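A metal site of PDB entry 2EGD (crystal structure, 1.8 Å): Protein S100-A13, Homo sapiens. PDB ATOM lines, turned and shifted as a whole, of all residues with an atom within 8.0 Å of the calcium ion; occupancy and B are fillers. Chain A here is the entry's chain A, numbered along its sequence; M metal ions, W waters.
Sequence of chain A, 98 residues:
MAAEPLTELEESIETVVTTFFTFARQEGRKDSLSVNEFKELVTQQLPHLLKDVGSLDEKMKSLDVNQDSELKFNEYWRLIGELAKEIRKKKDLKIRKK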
ATOM      1  N   PHE A  20     -25.441 -23.961  31.957  1.00  0.00           N
ATOM      2  CA  PHE A  20     -24.522 -23.531  30.861  1.00  0.00           C
ATOM      3  C   PHE A  20     -25.219 -22.523  29.936  1.00  0.00           C
ATOM      4  O   PHE A  20     -24.698 -21.427  29.699  1.00  0.00           O
ATOM      5  CB  PHE A  20     -24.084 -24.727  30.029  1.00  0.00           C
ATOM      6  CG  PHE A  20     -23.229 -24.365  28.855  1.00  0.00           C
ATOM      7  CD1 PHE A  20     -21.854 -24.143  29.024  1.00  0.00           C
ATOM      8  CD2 PHE A  20     -23.793 -24.227  27.568  1.00  0.00           C
ATOM      9  CE1 PHE A  20     -21.049 -23.827  27.881  1.00  0.00           C
ATOM     10  CE2 PHE A  20     -23.039 -23.880  26.456  1.00  0.00           C
ATOM     11  CZ  PHE A  20     -21.644 -23.679  26.584  1.00  0.00           C
ATOM     12  N   PHE A  21     -26.414 -22.856  29.458  1.00  0.00           N
ATOM     13  CA  PHE A  21     -27.081 -22.012  28.484  1.00  0.00           C
ATOM     14  C   PHE A  21     -27.573 -20.705  29.093  1.00  0.00           C
ATOM     15  O   PHE A  21     -27.564 -19.662  28.432  1.00  0.00           O
ATOM     16  CB  PHE A  21     -28.182 -22.803  27.775  1.00  0.00           C
ATOM     17  CG  PHE A  21     -27.600 -23.849  26.857  1.00  0.00           C
ATOM     18  CD1 PHE A  21     -26.966 -23.450  25.676  1.00  0.00           C
ATOM     19  CD2 PHE A  21     -27.566 -25.174  27.235  1.00  0.00           C
ATOM     20  CE1 PHE A  21     -26.428 -24.386  24.820  1.00  0.00           C
ATOM     21  CE2 PHE A  21     -26.990 -26.124  26.400  1.00  0.00           C
ATOM     22  CZ  PHE A  21     -26.421 -25.719  25.194  1.00  0.00           C
ATOM     23  N   THR A  22     -27.965 -20.756  30.356  1.00  0.00           N
ATOM     24  CA  THR A  22     -28.306 -19.530  31.081  1.00  0.00           C
ATOM     25  C   THR A  22     -27.206 -18.527  31.094  1.00  0.00           C
ATOM     26  O   THR A  22     -27.438 -17.347  30.795  1.00  0.00           O
ATOM     27  CB  THR A  22     -28.792 -19.814  32.522  1.00  0.00           C
ATOM     28  OG1 THR A  22     -30.017 -20.537  32.438  1.00  0.00           O
ATOM     29  CG2 THR A  22     -29.119 -18.480  33.323  1.00  0.00           C
ATOM     30  N   PHE A  23     -25.993 -18.994  31.419  1.00  0.00           N
ATOM     31  CA  PHE A  23     -24.821 -18.109  31.357  1.00  0.00           C
ATOM     32  C   PHE A  23     -24.277 -17.787  29.949  1.00  0.00           C
ATOM     33  O   PHE A  23     -23.842 -16.663  29.728  1.00  0.00           O
ATOM     34  CB  PHE A  23     -23.729 -18.607  32.308  1.00  0.00           C
ATOM     35  CG  PHE A  23     -24.106 -18.346  33.746  1.00  0.00           C
ATOM     36  CD1 PHE A  23     -23.704 -17.172  34.390  1.00  0.00           C
ATOM     37  CD2 PHE A  23     -24.889 -19.264  34.440  1.00  0.00           C
ATOM     38  CE1 PHE A  23     -24.077 -16.907  35.745  1.00  0.00           C
ATOM     39  CE2 PHE A  23     -25.311 -18.999  35.774  1.00  0.00           C
ATOM     40  CZ  PHE A  23     -24.896 -17.795  36.459  1.00  0.00           C
ATOM     41  N   ALA A  24     -24.400 -18.710  29.008  1.00  0.00           N
ATOM     42  CA  ALA A  24     -23.806 -18.583  27.687  1.00  0.00           C
ATOM     43  C   ALA A  24     -24.579 -17.621  26.811  1.00  0.00           C
ATOM     44  O   ALA A  24     -24.073 -17.142  25.816  1.00  0.00           O
ATOM     45  CB  ALA A  24     -23.693 -19.979  26.996  1.00  0.00           C
ATOM     46  N   ARG A  25     -25.820 -17.321  27.176  1.00  0.00           N
ATOM     47  CA  ARG A  25     -26.624 -16.456  26.268  1.00  0.00           C
ATOM     48  C   ARG A  25     -26.493 -14.969  26.589  1.00  0.00           C
ATOM     49  O   ARG A  25     -27.163 -14.129  25.989  1.00  0.00           O
ATOM     50  CB  ARG A  25     -28.092 -16.889  26.277  1.00  0.00           C
ATOM     51  CG  ARG A  25     -28.819 -16.589  27.570  1.00  0.00           C
ATOM     52  CD  ARG A  25     -30.316 -16.865  27.432  1.00  0.00           C
ATOM     53  NE  ARG A  25     -30.567 -18.166  26.811  1.00  0.00           N
ATOM     54  CZ  ARG A  25     -30.920 -19.265  27.479  1.00  0.00           C
ATOM     55  NH1 ARG A  25     -31.108 -19.230  28.797  1.00  0.00           N
ATOM     56  NH2 ARG A  25     -31.147 -20.399  26.789  1.00  0.00           N
ATOM     57  N   GLN A  26     -25.614 -14.645  27.532  1.00  0.00           N
ATOM     58  CA  GLN A  26     -25.534 -13.257  28.007  1.00  0.00           C
ATOM     59  C   GLN A  26     -24.848 -12.314  27.007  1.00  0.00           C
ATOM     60  O   GLN A  26     -25.214 -11.126  26.885  1.00  0.00           O
ATOM     61  CB  GLN A  26     -24.931 -13.176  29.411  1.00  0.00           C
ATOM     62  CG  GLN A  26     -25.735 -13.913  30.547  1.00  0.00           C
ATOM     63  CD  GLN A  26     -27.208 -13.495  30.658  1.00  0.00           C
ATOM     64  OE1 GLN A  26     -27.511 -12.306  30.757  1.00  0.00           O
ATOM     65  NE2 GLN A  26     -28.121 -14.478  30.656  1.00  0.00           N
ATOM     66  N   GLU A  27     -23.890 -12.841  26.268  1.00  0.00           N
ATOM     67  CA  GLU A  27     -23.165 -12.042  25.268  1.00  0.00           C
ATOM     68  C   GLU A  27     -22.560 -12.943  24.190  1.00  0.00           C
ATOM     69  O   GLU A  27     -22.322 -14.135  24.426  1.00  0.00           O
ATOM     70  CB  GLU A  27     -22.063 -11.223  25.962  1.00  0.00           C
ATOM     71  CG  GLU A  27     -20.974 -12.068  26.631  1.00  0.00           C
ATOM     72  CD  GLU A  27     -19.920 -11.241  27.325  1.00  0.00           C
ATOM     73  OE1 GLU A  27     -20.246 -10.147  27.835  1.00  0.00           O
ATOM     74  OE2 GLU A  27     -18.745 -11.684  27.359  1.00  0.00           O
ATOM     75  N   GLY A  28     -22.297 -12.376  23.017  1.00  0.00           N
ATOM     76  CA  GLY A  28     -21.715 -13.115  21.891  1.00  0.00           C
ATOM     77  C   GLY A  28     -22.551 -14.332  21.531  1.00  0.00           C
ATOM     78  O   GLY A  28     -23.769 -14.250  21.620  1.00  0.00           O
ATOM     79  N   ARG A  29     -21.889 -15.438  21.162  1.00  0.00           N
ATOM     80  CA  ARG A  29     -22.576 -16.657  20.718  1.00  0.00           C
ATOM     81  C   ARG A  29     -23.369 -17.229  21.874  1.00  0.00           C
ATOM     82  O   ARG A  29     -22.865 -17.307  22.983  1.00  0.00           O
ATOM     83  CB  ARG A  29     -21.568 -17.707  20.220  1.00  0.00           C
ATOM     84  CG  ARG A  29     -21.092 -17.540  18.797  1.00  0.00           C
ATOM     85  CD  ARG A  29     -21.929 -18.395  17.816  1.00  0.00           C
ATOM     86  N   LYS A  30     -24.593 -17.641  21.618  1.00  0.00           N
ATOM     87  CA  LYS A  30     -25.446 -18.072  22.724  1.00  0.00           C
ATOM     88  C   LYS A  30     -25.143 -19.512  23.158  1.00  0.00           C
ATOM     89  O   LYS A  30     -25.696 -19.979  24.190  1.00  0.00           O
ATOM     90  CB  LYS A  30     -26.925 -17.901  22.355  1.00  0.00           C
ATOM     91  CG  LYS A  30     -27.503 -19.101  21.590  1.00  0.00           C
ATOM     92  N   ASP A  31     -24.274 -20.199  22.408  1.00  0.00           N
ATOM     93  CA  ASP A  31     -23.942 -21.612  22.689  1.00  0.00           C
ATOM     94  C   ASP A  31     -22.520 -21.740  23.244  1.00  0.00           C
ATOM     95  O   ASP A  31     -21.952 -22.851  23.309  1.00  0.00           O
ATOM     96  CB  ASP A  31     -24.131 -22.507  21.434  1.00  0.00           C
ATOM     97  CG  ASP A  31     -23.181 -22.173  20.291  1.00  0.00           C
ATOM     98  OD1 ASP A  31     -22.477 -21.132  20.307  1.00  0.00           O
ATOM     99  OD2 ASP A  31     -23.165 -22.941  19.345  1.00  0.00           O
ATOM    100  N   SER A  32     -21.945 -20.626  23.662  1.00  0.00           N
ATOM    101  CA  SER A  32     -20.631 -20.693  24.308  1.00  0.00           C
ATOM    102  C   SER A  32     -20.433 -19.618  25.365  1.00  0.00           C
ATOM    103  O   SER A  32     -21.055 -18.551  25.308  1.00  0.00           O
ATOM    104  CB  SER A  32     -19.488 -20.742  23.301  1.00  0.00           C
ATOM    105  OG  SER A  32     -19.299 -19.484  22.733  1.00  0.00           O
ATOM    106  N   LEU A  33     -19.591 -19.939  26.344  1.00  0.00           N
ATOM    107  CA  LEU A  33     -19.216 -19.027  27.428  1.00  0.00           C
ATOM    108  C   LEU A  33     -17.967 -18.225  27.030  1.00  0.00           C
ATOM    109  O   LEU A  33     -16.914 -18.818  26.753  1.00  0.00           O
ATOM    110  CB  LEU A  33     -18.871 -19.848  28.694  1.00  0.00           C
ATOM    111  CG  LEU A  33     -20.047 -20.599  29.293  1.00  0.00           C
ATOM    112  CD1 LEU A  33     -19.486 -21.548  30.356  1.00  0.00           C
ATOM    113  CD2 LEU A  33     -21.102 -19.731  29.895  1.00  0.00           C
ATOM    114  N   SER A  34     -18.079 -16.885  26.986  1.00  0.00           N
ATOM    115  CA  SER A  34     -16.883 -16.027  26.923  1.00  0.00           C
ATOM    116  C   SER A  34     -16.234 -16.053  28.303  1.00  0.00           C
ATOM    117  O   SER A  34     -16.802 -16.597  29.255  1.00  0.00           O
ATOM    118  CB  SER A  34     -17.310 -14.591  26.626  1.00  0.00           C
ATOM    119  OG  SER A  34     -18.056 -14.142  27.769  1.00  0.00           O
ATOM    120  N   VAL A  35     -15.059 -15.465  28.416  1.00  0.00           N
ATOM    121  CA  VAL A  35     -14.426 -15.355  29.757  1.00  0.00           C
ATOM    122  C   VAL A  35     -15.311 -14.656  30.789  1.00  0.00           C
ATOM    123  O   VAL A  35     -15.361 -15.085  31.943  1.00  0.00           O
ATOM    124  CB  VAL A  35     -13.055 -14.669  29.700  1.00  0.00           C
ATOM    125  CG1 VAL A  35     -13.200 -13.205  29.305  1.00  0.00           C
ATOM    126  CG2 VAL A  35     -12.340 -14.803  31.068  1.00  0.00           C
ATOM    127  N   GLU A  37     -18.645 -14.506  30.867  1.00  0.00           N
ATOM    128  CA  GLU A  37     -19.759 -15.423  31.212  1.00  0.00           C
ATOM    129  C   GLU A  37     -19.292 -16.590  32.114  1.00  0.00           C
ATOM    130  O   GLU A  37     -20.015 -17.028  33.018  1.00  0.00           O
ATOM    131  CB  GLU A  37     -20.394 -15.974  29.930  1.00  0.00           C
ATOM    132  CG  GLU A  37     -21.099 -14.897  29.103  1.00  0.00           C
ATOM    133  CD  GLU A  37     -21.529 -15.397  27.750  1.00  0.00           C
ATOM    134  OE1 GLU A  37     -20.787 -16.210  27.166  1.00  0.00           O
ATOM    135  OE2 GLU A  37     -22.641 -15.025  27.304  1.00  0.00           O
ATOM    136  N   PHE A  38     -18.095 -17.076  31.840  1.00  0.00           N
ATOM    137  CA  PHE A  38     -17.496 -18.160  32.635  1.00  0.00           C
ATOM    138  C   PHE A  38     -17.257 -17.637  34.009  1.00  0.00           C
ATOM    139  O   PHE A  38     -17.560 -18.296  34.995  1.00  0.00           O
ATOM    140  CB  PHE A  38     -16.152 -18.564  32.007  1.00  0.00           C
ATOM    141  CG  PHE A  38     -15.339 -19.446  32.892  1.00  0.00           C
ATOM    142  CD1 PHE A  38     -15.774 -20.764  33.181  1.00  0.00           C
ATOM    143  CD2 PHE A  38     -14.148 -18.987  33.475  1.00  0.00           C
ATOM    144  CE1 PHE A  38     -15.001 -21.618  34.024  1.00  0.00           C
ATOM    145  CE2 PHE A  38     -13.400 -19.813  34.319  1.00  0.00           C
ATOM    146  CZ  PHE A  38     -13.827 -21.132  34.602  1.00  0.00           C
ATOM    147  N   GLU A  70     -13.372 -19.369  24.013  1.00  0.00           N
ATOM    148  CA  GLU A  70     -14.750 -19.629  24.448  1.00  0.00           C
ATOM    149  C   GLU A  70     -14.867 -21.035  25.010  1.00  0.00           C
ATOM    150  O   GLU A  70     -14.140 -21.908  24.601  1.00  0.00           O
ATOM    151  CB  GLU A  70     -15.756 -19.501  23.275  1.00  0.00           C
ATOM    152  CG  GLU A  70     -15.728 -18.165  22.560  1.00  0.00           C
ATOM    153  CD  GLU A  70     -16.821 -17.182  22.966  1.00  0.00           C
ATOM    154  OE1 GLU A  70     -16.608 -15.987  22.773  1.00  0.00           O
ATOM    155  OE2 GLU A  70     -17.897 -17.586  23.452  1.00  0.00           O
ATOM    156  N   LEU A  71     -15.814 -21.253  25.928  1.00  0.00           N
ATOM    157  CA  LEU A  71     -16.075 -22.623  26.367  1.00  0.00           C
ATOM    158  C   LEU A  71     -17.396 -23.093  25.732  1.00  0.00           C
ATOM    159  O   LEU A  71     -18.448 -22.546  26.062  1.00  0.00           O
ATOM    160  CB  LEU A  71     -16.199 -22.698  27.903  1.00  0.00           C
ATOM    161  CG  LEU A  71     -14.952 -22.186  28.644  1.00  0.00           C
ATOM    162  CD1 LEU A  71     -15.027 -22.541  30.103  1.00  0.00           C
ATOM    163  CD2 LEU A  71     -13.664 -22.750  27.983  1.00  0.00           C
HETATM  164 CA    CA M   1     -21.972 -16.416  25.108  1.00  0.00          CA
HETATM  165  O   HOH W   1     -19.839 -15.924  24.045  1.00  0.00           O
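The side-chain hydroxyl (OG) of Ser 32 is in hydrogen-bond range of the side-chain carboxylate (OE2) of Glu 70 (2.5 Å). OG of Ser 34 is in hydrogen-bond range of N of Glu 37, 3.2 Å away. OE2 of Glu 37 sits close to N of Gln 26. The side-chain carboxylate (OE2) of Glu 27 sits at hydrogen-bond distance from the side-chain hydroxyl (OG) of Ser 34, at 2.6 Å.
Five residues have an atom within 4 Å of the calcium ion: Ala 24, Glu 27, Arg 29, Ser 32 and Glu 37.
The calcium ion is bound by O of Ser 32 (2.3 Å), O of Ala 24 (2.3 Å), OE1 of Glu 37 (2.4 Å), O of Glu 27 (2.4 Å), water W1 (2.4 Å), O of Arg 29 (2.5 Å) and OE2 of Glu 37 (2.7 Å).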
